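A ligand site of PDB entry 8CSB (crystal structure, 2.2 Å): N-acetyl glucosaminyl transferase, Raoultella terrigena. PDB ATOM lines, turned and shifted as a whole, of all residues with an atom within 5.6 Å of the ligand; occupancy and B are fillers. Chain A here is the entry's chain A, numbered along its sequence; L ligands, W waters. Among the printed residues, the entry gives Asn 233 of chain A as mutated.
OG of Ser 286 lies within hydrogen-bond range of OE1 of Glu 306. OE1 of Gln 229 lies within hydrogen-bond range of N of Asn 300 (3.0 Å). OE1 of Gln 229 lies within hydrogen-bond range of N of Ser 301, at 3.2 Å. The backbone carbonyl oxygen (O) of Glu 159 is in hydrogen-bond range of the backbone NH (N) of Tyr 173 (2.8 Å). The side-chain amide oxygen (OD1) of Asn 233 lies close to the backbone NH (N) of Asn 235 (3.3 Å). OG of Ser 301 is in hydrogen-bond range of N of Val 303, at 2.9 Å. The guanidinium group (NE) of Arg 164 lies within hydrogen-bond range of the backbone carbonyl oxygen (O) of Gly 161, at 2.8 Å. The backbone carbonyl oxygen (O) of Asn 300 lies within hydrogen-bond range of the side-chain amide nitrogen (ND2) of Asn 235, at 3.1 Å.
N2 of the ligand sits at hydrogen-bond distance from NE of Arg 264 (2.9 Å). O11 of the ligand lies close to OD1 of Asn 233. The side-chain hydroxyl (OG) of Ser 302 is in hydrogen-bond range of an oxygen (O6) of the ligand (2.6 Å). OE2 of Glu 159 sits close to O14 of the ligand (3.2 Å). The side-chain amide nitrogen (ND2) of Asn 235 sits at hydrogen-bond distance from an oxygen (O11) of the ligand. A ring nitrogen (NE2) of His 266 lies within hydrogen-bond range of an oxygen (O9) of the ligand (3.1 Å). NE2 of Gln 229 sits at hydrogen-bond distance from O11 of the ligand (2.5 Å). NH2 of Arg 164 is in hydrogen-bond range of O13 of the ligand (2.9 Å). The backbone NH (N) of Ser 302 lies within hydrogen-bond range of an oxygen (O6) of the ligand (2.7 Å). The side-chain hydroxyl (OG) of Ser 301 is in hydrogen-bond range of an oxygen (O7) of the ligand (2.6 Å). The backbone carbonyl oxygen of Leu 228 lies within hydrogen-bond range of a nitrogen (N3) of the ligand. N3 of the ligand lies within hydrogen-bond range of O of Ala 265. An oxygen (O12) of the ligand sits at hydrogen-bond distance from the backbone NH of Val 230, 3.1 Å away. O of Arg 264 lies within hydrogen-bond range of N3 of the ligand, 3.1 Å away. ND2 of Asn 180 is in hydrogen-bond range of O14 of the ligand, at 2.8 Å.
Water W2 lies within hydrogen-bond range of the backbone NH of Ser 286 (2.5 Å) and an oxygen (O2) of the ligand (3.1 Å). Water W1 lies within hydrogen-bond range of the backbone NH (N) of Arg 164 (2.9 Å), the backbone carbonyl oxygen (O) of Pro 162 (3.0 Å) and an oxygen (O4) of the ligand (3.3 Å).
Residues that only touch the ligand: Pro 162 (3.9 Å), Val 227 (3.6 Å), Pro 267 (3.7 Å), Ser 286 (3.2 Å) and Val 303 (3.6 Å). Of the 27 residues printed, 18 come within 4 Å of the ligand. The nearest printed residue that does not touch the ligand is Ile 160 (4.1 Å).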
ATOM      1  N   GLU A 159      19.097  -8.282 -32.139  1.00  0.00           N
ATOM      2  CA  GLU A 159      18.980  -8.428 -30.699  1.00  0.00           C
ATOM      3  C   GLU A 159      18.956  -9.913 -30.449  1.00  0.00           C
ATOM      4  O   GLU A 159      18.665 -10.697 -31.352  1.00  0.00           O
ATOM      5  CB  GLU A 159      17.682  -7.731 -30.185  1.00  0.00           C
ATOM      6  CG  GLU A 159      17.377  -7.641 -28.695  1.00  0.00           C
ATOM      7  CD  GLU A 159      18.519  -7.126 -27.791  1.00  0.00           C
ATOM      8  OE1 GLU A 159      19.593  -7.765 -27.718  1.00  0.00           O
ATOM      9  OE2 GLU A 159      18.335  -6.114 -27.093  1.00  0.00           O
ATOM     10  N   ILE A 160      19.331 -10.303 -29.204  1.00  0.00           N
ATOM     11  CA  ILE A 160      19.143 -11.684 -28.792  1.00  0.00           C
ATOM     12  C   ILE A 160      17.661 -12.066 -28.912  1.00  0.00           C
ATOM     13  O   ILE A 160      16.743 -11.246 -28.684  1.00  0.00           O
ATOM     14  CB  ILE A 160      19.654 -11.915 -27.363  1.00  0.00           C
ATOM     15  CG1 ILE A 160      19.709 -13.438 -27.088  1.00  0.00           C
ATOM     16  CG2 ILE A 160      18.802 -11.175 -26.288  1.00  0.00           C
ATOM     17  CD1 ILE A 160      20.585 -13.844 -25.912  1.00  0.00           C
ATOM     18  N   GLY A 161      17.438 -13.342 -29.309  1.00  0.00           N
ATOM     19  CA  GLY A 161      16.107 -13.822 -29.608  1.00  0.00           C
ATOM     20  C   GLY A 161      15.299 -14.163 -28.364  1.00  0.00           C
ATOM     21  O   GLY A 161      15.761 -14.011 -27.225  1.00  0.00           O
ATOM     22  N   PRO A 162      14.052 -14.622 -28.569  1.00  0.00           N
ATOM     23  CA  PRO A 162      13.240 -15.066 -27.422  1.00  0.00           C
ATOM     24  C   PRO A 162      13.540 -16.509 -26.967  1.00  0.00           C
ATOM     25  O   PRO A 162      13.104 -16.875 -25.864  1.00  0.00           O
ATOM     26  CB  PRO A 162      11.809 -14.940 -27.946  1.00  0.00           C
ATOM     27  CG  PRO A 162      11.965 -15.213 -29.547  1.00  0.00           C
ATOM     28  CD  PRO A 162      13.424 -14.881 -29.885  1.00  0.00           C
ATOM     29  N   ARG A 164      16.699 -19.066 -25.969  1.00  0.00           N
ATOM     30  CA  ARG A 164      18.090 -18.850 -25.555  1.00  0.00           C
ATOM     31  C   ARG A 164      18.681 -20.074 -24.853  1.00  0.00           C
ATOM     32  O   ARG A 164      17.963 -20.834 -24.202  1.00  0.00           O
ATOM     33  CB  ARG A 164      18.192 -17.645 -24.604  1.00  0.00           C
ATOM     34  CG  ARG A 164      17.518 -16.364 -25.190  1.00  0.00           C
ATOM     35  CD  ARG A 164      17.475 -15.241 -24.162  1.00  0.00           C
ATOM     36  NE  ARG A 164      16.726 -14.078 -24.581  1.00  0.00           N
ATOM     37  CZ  ARG A 164      16.534 -13.019 -23.819  1.00  0.00           C
ATOM     38  NH1 ARG A 164      17.018 -12.960 -22.587  1.00  0.00           N
ATOM     39  NH2 ARG A 164      15.860 -11.987 -24.301  1.00  0.00           N
ATOM     40  N   TYR A 173      17.116 -11.959 -33.253  1.00  0.00           N
ATOM     41  CA  TYR A 173      16.222 -11.226 -34.146  1.00  0.00           C
ATOM     42  C   TYR A 173      17.040 -10.549 -35.233  1.00  0.00           C
ATOM     43  O   TYR A 173      18.172 -10.125 -34.984  1.00  0.00           O
ATOM     44  CB  TYR A 173      15.451 -10.146 -33.416  1.00  0.00           C
ATOM     45  CG  TYR A 173      14.419 -10.617 -32.430  1.00  0.00           C
ATOM     46  CD1 TYR A 173      13.301 -11.285 -32.865  1.00  0.00           C
ATOM     47  CD2 TYR A 173      14.535 -10.301 -31.074  1.00  0.00           C
ATOM     48  CE1 TYR A 173      12.317 -11.658 -31.990  1.00  0.00           C
ATOM     49  CE2 TYR A 173      13.555 -10.682 -30.164  1.00  0.00           C
ATOM     50  CZ  TYR A 173      12.432 -11.366 -30.642  1.00  0.00           C
ATOM     51  OH  TYR A 173      11.433 -11.800 -29.788  1.00  0.00           O
ATOM     52  N   VAL A 179      13.055  -3.984 -34.136  1.00  0.00           N
ATOM     53  CA  VAL A 179      13.252  -5.112 -33.225  1.00  0.00           C
ATOM     54  C   VAL A 179      12.353  -4.878 -32.016  1.00  0.00           C
ATOM     55  O   VAL A 179      12.304  -3.764 -31.474  1.00  0.00           O
ATOM     56  CB  VAL A 179      14.746  -5.252 -32.840  1.00  0.00           C
ATOM     57  CG1 VAL A 179      15.236  -4.001 -32.119  1.00  0.00           C
ATOM     58  CG2 VAL A 179      15.047  -6.552 -32.049  1.00  0.00           C
ATOM     59  N   ASN A 180      11.565  -5.904 -31.646  1.00  0.00           N
ATOM     60  CA  ASN A 180      10.531  -5.795 -30.604  1.00  0.00           C
ATOM     61  C   ASN A 180       9.317  -4.952 -30.986  1.00  0.00           C
ATOM     62  O   ASN A 180       8.182  -5.474 -31.060  1.00  0.00           O
ATOM     63  CB  ASN A 180      11.153  -5.251 -29.308  1.00  0.00           C
ATOM     64  CG  ASN A 180      12.097  -6.252 -28.704  1.00  0.00           C
ATOM     65  OD1 ASN A 180      11.850  -7.445 -28.798  1.00  0.00           O
ATOM     66  ND2 ASN A 180      13.197  -5.778 -28.132  1.00  0.00           N
ATOM     67  N   VAL A 227       3.274 -13.263 -16.037  1.00  0.00           N
ATOM     68  CA  VAL A 227       4.698 -13.101 -16.340  1.00  0.00           C
ATOM     69  C   VAL A 227       5.102 -11.671 -16.059  1.00  0.00           C
ATOM     70  O   VAL A 227       4.613 -10.761 -16.733  1.00  0.00           O
ATOM     71  CB  VAL A 227       5.013 -13.395 -17.809  1.00  0.00           C
ATOM     72  CG1 VAL A 227       6.494 -13.015 -18.082  1.00  0.00           C
ATOM     73  CG2 VAL A 227       4.651 -14.875 -18.177  1.00  0.00           C
ATOM     74  N   LEU A 228       6.065 -11.460 -15.171  1.00  0.00           N
ATOM     75  CA  LEU A 228       6.546 -10.094 -14.979  1.00  0.00           C
ATOM     76  C   LEU A 228       7.832  -9.900 -15.791  1.00  0.00           C
ATOM     77  O   LEU A 228       8.485 -10.865 -16.178  1.00  0.00           O
ATOM     78  CB  LEU A 228       6.738  -9.798 -13.489  1.00  0.00           C
ATOM     79  CG  LEU A 228       5.516 -10.068 -12.577  1.00  0.00           C
ATOM     80  CD1 LEU A 228       5.705  -9.483 -11.181  1.00  0.00           C
ATOM     81  CD2 LEU A 228       4.213  -9.557 -13.249  1.00  0.00           C
ATOM     82  N   GLN A 229       8.147  -8.631 -16.112  1.00  0.00           N
ATOM     83  CA  GLN A 229       9.299  -8.343 -16.938  1.00  0.00           C
ATOM     84  C   GLN A 229      10.221  -7.382 -16.213  1.00  0.00           C
ATOM     85  O   GLN A 229       9.878  -6.842 -15.166  1.00  0.00           O
ATOM     86  CB  GLN A 229       8.874  -7.742 -18.295  1.00  0.00           C
ATOM     87  CG  GLN A 229       8.160  -8.788 -19.127  1.00  0.00           C
ATOM     88  CD  GLN A 229       7.713  -8.222 -20.432  1.00  0.00           C
ATOM     89  OE1 GLN A 229       6.519  -8.155 -20.679  1.00  0.00           O
ATOM     90  NE2 GLN A 229       8.669  -7.804 -21.292  1.00  0.00           N
ATOM     91  N   VAL A 230      11.405  -7.164 -16.779  1.00  0.00           N
ATOM     92  CA  VAL A 230      12.271  -6.128 -16.221  1.00  0.00           C
ATOM     93  C   VAL A 230      11.641  -4.761 -16.433  1.00  0.00           C
ATOM     94  O   VAL A 230      11.141  -4.438 -17.524  1.00  0.00           O
ATOM     95  CB  VAL A 230      13.699  -6.200 -16.770  1.00  0.00           C
ATOM     96  CG1 VAL A 230      14.618  -5.166 -15.988  1.00  0.00           C
ATOM     97  CG2 VAL A 230      14.298  -7.667 -16.534  1.00  0.00           C
ATOM     98  N   ASN A 233      13.100  -2.317 -19.071  1.00  0.00           N
ATOM     99  CA  ASN A 233      13.481  -2.869 -20.361  1.00  0.00           C
ATOM    100  C   ASN A 233      12.815  -2.080 -21.506  1.00  0.00           C
ATOM    101  O   ASN A 233      11.700  -1.583 -21.365  1.00  0.00           O
ATOM    102  CB  ASN A 233      13.076  -4.341 -20.413  1.00  0.00           C
ATOM    103  CG  ASN A 233      13.727  -5.099 -21.559  1.00  0.00           C
ATOM    104  OD1 ASN A 233      13.126  -5.282 -22.650  1.00  0.00           O
ATOM    105  ND2 ASN A 233      14.967  -5.523 -21.354  1.00  0.00           N
ATOM    106  N   SER A 234      13.514  -1.972 -22.661  1.00  0.00           N
ATOM    107  CA  SER A 234      12.961  -1.268 -23.832  1.00  0.00           C
ATOM    108  C   SER A 234      11.524  -1.709 -24.139  1.00  0.00           C
ATOM    109  O   SER A 234      10.657  -0.854 -24.327  1.00  0.00           O
ATOM    110  CB  SER A 234      13.886  -1.450 -25.050  1.00  0.00           C
ATOM    111  OG  SER A 234      13.859  -2.760 -25.605  1.00  0.00           O
ATOM    112  N   ASN A 235      11.247  -3.033 -24.088  1.00  0.00           N
ATOM    113  CA  ASN A 235       9.904  -3.633 -24.182  1.00  0.00           C
ATOM    114  C   ASN A 235       8.862  -3.005 -23.261  1.00  0.00           C
ATOM    115  O   ASN A 235       7.679  -2.883 -23.641  1.00  0.00           O
ATOM    116  CB  ASN A 235       9.971  -5.119 -23.804  1.00  0.00           C
ATOM    117  CG  ASN A 235      10.388  -5.974 -24.913  1.00  0.00           C
ATOM    118  OD1 ASN A 235      10.992  -5.510 -25.879  1.00  0.00           O
ATOM    119  ND2 ASN A 235      10.074  -7.254 -24.829  1.00  0.00           N
ATOM    120  N   LEU A 236       9.240  -2.733 -22.019  1.00  0.00           N
ATOM    121  CA  LEU A 236       8.349  -2.135 -21.016  1.00  0.00           C
ATOM    122  C   LEU A 236       8.326  -0.606 -21.016  1.00  0.00           C
ATOM    123  O   LEU A 236       7.489  -0.001 -20.322  1.00  0.00           O
ATOM    124  CB  LEU A 236       8.743  -2.632 -19.615  1.00  0.00           C
ATOM    125  CG  LEU A 236       7.508  -3.341 -19.108  1.00  0.00           C
ATOM    126  CD1 LEU A 236       7.356  -4.560 -19.970  1.00  0.00           C
ATOM    127  CD2 LEU A 236       7.751  -3.688 -17.688  1.00  0.00           C
ATOM    128  N   ARG A 264       5.265 -15.082 -11.612  1.00  0.00           N
ATOM    129  CA  ARG A 264       6.713 -15.247 -11.752  1.00  0.00           C
ATOM    130  C   ARG A 264       7.374 -13.880 -12.020  1.00  0.00           C
ATOM    131  O   ARG A 264       7.234 -13.315 -13.120  1.00  0.00           O
ATOM    132  CB  ARG A 264       7.046 -16.242 -12.861  1.00  0.00           C
ATOM    133  CG  ARG A 264       8.555 -16.412 -13.040  1.00  0.00           C
ATOM    134  CD  ARG A 264       8.909 -17.554 -13.974  1.00  0.00           C
ATOM    135  NE  ARG A 264      10.338 -17.656 -14.236  1.00  0.00           N
ATOM    136  CZ  ARG A 264      11.205 -18.356 -13.507  1.00  0.00           C
ATOM    137  NH1 ARG A 264      10.828 -19.022 -12.413  1.00  0.00           N
ATOM    138  NH2 ARG A 264      12.496 -18.380 -13.858  1.00  0.00           N
ATOM    139  N   ALA A 265       8.097 -13.374 -11.027  1.00  0.00           N
ATOM    140  CA  ALA A 265       8.986 -12.251 -11.254  1.00  0.00           C
ATOM    141  C   ALA A 265      10.056 -12.622 -12.285  1.00  0.00           C
ATOM    142  O   ALA A 265      10.365 -13.811 -12.504  1.00  0.00           O
ATOM    143  CB  ALA A 265       9.602 -11.812  -9.936  1.00  0.00           C
ATOM    144  N   HIS A 266      10.572 -11.599 -13.003  1.00  0.00           N
ATOM    145  CA  HIS A 266      11.726 -11.784 -13.901  1.00  0.00           C
ATOM    146  C   HIS A 266      12.981 -11.950 -13.047  1.00  0.00           C
ATOM    147  O   HIS A 266      13.279 -11.061 -12.255  1.00  0.00           O
ATOM    148  CB  HIS A 266      11.901 -10.553 -14.872  1.00  0.00           C
ATOM    149  CG  HIS A 266      12.821 -10.806 -16.050  1.00  0.00           C
ATOM    150  ND1 HIS A 266      14.183 -11.003 -15.918  1.00  0.00           N
ATOM    151  CD2 HIS A 266      12.558 -10.892 -17.386  1.00  0.00           C
ATOM    152  CE1 HIS A 266      14.721 -11.200 -17.116  1.00  0.00           C
ATOM    153  NE2 HIS A 266      13.755 -11.134 -18.017  1.00  0.00           N
ATOM    154  N   PRO A 267      13.728 -13.065 -13.151  1.00  0.00           N
ATOM    155  CA  PRO A 267      15.027 -13.159 -12.431  1.00  0.00           C
ATOM    156  C   PRO A 267      15.890 -11.926 -12.581  1.00  0.00           C
ATOM    157  O   PRO A 267      16.591 -11.564 -11.657  1.00  0.00           O
ATOM    158  CB  PRO A 267      15.702 -14.371 -13.101  1.00  0.00           C
ATOM    159  CG  PRO A 267      14.620 -15.267 -13.478  1.00  0.00           C
ATOM    160  CD  PRO A 267      13.438 -14.302 -13.909  1.00  0.00           C
ATOM    161  N   ASN A 285      13.032 -22.319 -13.846  1.00  0.00           N
ATOM    162  CA  ASN A 285      13.095 -21.813 -15.206  1.00  0.00           C
ATOM    163  C   ASN A 285      11.678 -21.509 -15.715  1.00  0.00           C
ATOM    164  O   ASN A 285      10.691 -22.039 -15.202  1.00  0.00           O
ATOM    165  CB  ASN A 285      13.827 -22.821 -16.099  1.00  0.00           C
ATOM    166  CG  ASN A 285      13.054 -24.082 -16.252  1.00  0.00           C
ATOM    167  OD1 ASN A 285      11.962 -24.094 -16.859  1.00  0.00           O
ATOM    168  ND2 ASN A 285      13.609 -25.177 -15.748  1.00  0.00           N
ATOM    169  N   SER A 286      11.564 -20.632 -16.720  1.00  0.00           N
ATOM    170  CA  SER A 286      10.196 -20.172 -17.060  1.00  0.00           C
ATOM    171  C   SER A 286       9.332 -21.271 -17.665  1.00  0.00           C
ATOM    172  O   SER A 286       8.094 -21.231 -17.554  1.00  0.00           O
ATOM    173  CB  SER A 286      10.208 -18.955 -18.000  1.00  0.00           C
ATOM    174  OG  SER A 286      10.839 -19.229 -19.233  1.00  0.00           O
ATOM    175  N   ASN A 300       4.826  -8.323 -23.118  1.00  0.00           N
ATOM    176  CA  ASN A 300       5.509  -8.764 -24.332  1.00  0.00           C
ATOM    177  C   ASN A 300       6.820  -9.504 -24.040  1.00  0.00           C
ATOM    178  O   ASN A 300       7.806  -9.333 -24.766  1.00  0.00           O
ATOM    179  CB  ASN A 300       5.753  -7.570 -25.289  1.00  0.00           C
ATOM    180  CG  ASN A 300       6.333  -6.356 -24.593  1.00  0.00           C
ATOM    181  OD1 ASN A 300       6.896  -6.486 -23.516  1.00  0.00           O
ATOM    182  ND2 ASN A 300       6.210  -5.152 -25.215  1.00  0.00           N
ATOM    183  N   SER A 301       6.837 -10.342 -23.002  1.00  0.00           N
ATOM    184  CA  SER A 301       8.026 -11.073 -22.602  1.00  0.00           C
ATOM    185  C   SER A 301       8.286 -12.248 -23.561  1.00  0.00           C
ATOM    186  O   SER A 301       7.353 -12.821 -24.111  1.00  0.00           O
ATOM    187  CB  SER A 301       7.852 -11.577 -21.163  1.00  0.00           C
ATOM    188  OG  SER A 301       8.576 -12.791 -20.885  1.00  0.00           O
ATOM    189  N   SER A 302       9.564 -12.589 -23.761  1.00  0.00           N
ATOM    190  CA  SER A 302       9.885 -13.832 -24.490  1.00  0.00           C
ATOM    191  C   SER A 302       9.106 -15.009 -23.971  1.00  0.00           C
ATOM    192  O   SER A 302       8.782 -15.917 -24.736  1.00  0.00           O
ATOM    193  CB  SER A 302      11.364 -14.144 -24.414  1.00  0.00           C
ATOM    194  OG  SER A 302      12.088 -12.986 -24.740  1.00  0.00           O
ATOM    195  N   VAL A 303       8.769 -15.033 -22.680  1.00  0.00           N
ATOM    196  CA  VAL A 303       8.091 -16.233 -22.120  1.00  0.00           C
ATOM    197  C   VAL A 303       6.716 -16.453 -22.757  1.00  0.00           C
ATOM    198  O   VAL A 303       6.214 -17.605 -22.774  1.00  0.00           O
ATOM    199  CB  VAL A 303       7.952 -16.145 -20.574  1.00  0.00           C
ATOM    200  CG1 VAL A 303       7.011 -17.260 -20.071  1.00  0.00           C
ATOM    201  CG2 VAL A 303       9.300 -16.117 -19.930  1.00  0.00           C
ATOM    202  N   GLU A 306       6.998 -18.976 -25.447  1.00  0.00           N
ATOM    203  CA  GLU A 306       7.097 -20.272 -24.797  1.00  0.00           C
ATOM    204  C   GLU A 306       5.718 -20.803 -24.427  1.00  0.00           C
ATOM    205  O   GLU A 306       5.379 -21.974 -24.688  1.00  0.00           O
ATOM    206  CB  GLU A 306       8.000 -20.052 -23.567  1.00  0.00           C
ATOM    207  CG  GLU A 306       8.702 -21.204 -23.005  1.00  0.00           C
ATOM    208  CD  GLU A 306       9.795 -20.831 -21.957  1.00  0.00           C
ATOM    209  OE1 GLU A 306       9.860 -19.662 -21.440  1.00  0.00           O
ATOM    210  OE2 GLU A 306      10.600 -21.725 -21.698  1.00  0.00           O
HETATM  211  N1  LIG L   1      12.182 -15.260 -17.796  1.00  0.00           N
HETATM  212  C1  LIG L   1      11.697 -15.953 -16.744  1.00  0.00           C
HETATM  213  N2  LIG L   1      10.626 -15.479 -16.062  1.00  0.00           N
HETATM  214  C2  LIG L   1      10.067 -14.322 -16.398  1.00  0.00           C
HETATM  215  C3  LIG L   1      10.562 -13.585 -17.442  1.00  0.00           C
HETATM  216  C4  LIG L   1      11.655 -14.078 -18.124  1.00  0.00           C
HETATM  217  O1  LIG L   1      12.141 -16.994 -16.412  1.00  0.00           O
HETATM  218  N3  LIG L   1       8.930 -13.890 -15.600  1.00  0.00           N
HETATM  219  C5  LIG L   1      13.234 -15.799 -18.426  1.00  0.00           C
HETATM  220  C6  LIG L   1      13.114 -16.627 -19.737  1.00  0.00           C
HETATM  221  O2  LIG L   1      14.340 -17.512 -19.687  1.00  0.00           O
HETATM  222  C7  LIG L   1      13.132 -15.761 -20.750  1.00  0.00           C
HETATM  223  C8  LIG L   1      14.157 -14.616 -20.175  1.00  0.00           C
HETATM  224  O3  LIG L   1      14.058 -14.559 -18.863  1.00  0.00           O
HETATM  225  O4  LIG L   1      13.512 -16.238 -22.073  1.00  0.00           O
HETATM  226  C9  LIG L   1      13.779 -13.329 -20.951  1.00  0.00           C
HETATM  227  O5  LIG L   1      12.341 -13.037 -21.113  1.00  0.00           O
HETATM  228  P1  LIG L   1      11.916 -11.401 -21.312  1.00  0.00           P
HETATM  229  O6  LIG L   1      11.744 -11.329 -22.784  1.00  0.00           O
HETATM  230  O7  LIG L   1      10.655 -11.242 -20.516  1.00  0.00           O
HETATM  231  O8  LIG L   1      13.366  -8.905 -22.872  1.00  0.00           O
HETATM  232  C10 LIG L   1      13.253  -8.971 -21.371  1.00  0.00           C
HETATM  233  O9  LIG L   1      13.138 -10.321 -20.894  1.00  0.00           O
HETATM  234  C11 LIG L   1      14.520  -8.422 -20.699  1.00  0.00           C
HETATM  235  C12 LIG L   1      15.728  -8.900 -21.386  1.00  0.00           C
HETATM  236  O10 LIG L   1      15.636 -10.325 -21.566  1.00  0.00           O
HETATM  237  C13 LIG L   1      15.798  -8.300 -22.748  1.00  0.00           C
HETATM  238  C14 LIG L   1      14.447  -8.017 -23.360  1.00  0.00           C
HETATM  239  C15 LIG L   1      14.472  -8.171 -24.861  1.00  0.00           C
HETATM  240  C16 LIG L   1      12.064  -8.192 -20.928  1.00  0.00           C
HETATM  241  O11 LIG L   1      11.133  -7.837 -21.762  1.00  0.00           O
HETATM  242  O12 LIG L   1      12.040  -7.962 -19.669  1.00  0.00           O
HETATM  243  O13 LIG L   1      16.468  -9.260 -23.575  1.00  0.00           O
HETATM  244  C17 LIG L   1      14.861  -6.797 -25.467  1.00  0.00           C
HETATM  245  O14 LIG L   1      15.314  -6.985 -26.789  1.00  0.00           O
HETATM  246  O15 LIG L   1      15.385  -9.215 -25.199  1.00  0.00           O
HETATM  247  O   HOH W   1      14.661 -18.661 -23.946  1.00  0.00           O
HETATM  248  O   HOH W   2      13.712 -19.724 -17.541  1.00  0.00           O
HETATM  249  O   HOH W   3      14.384 -19.655 -21.394  1.00  0.00           O
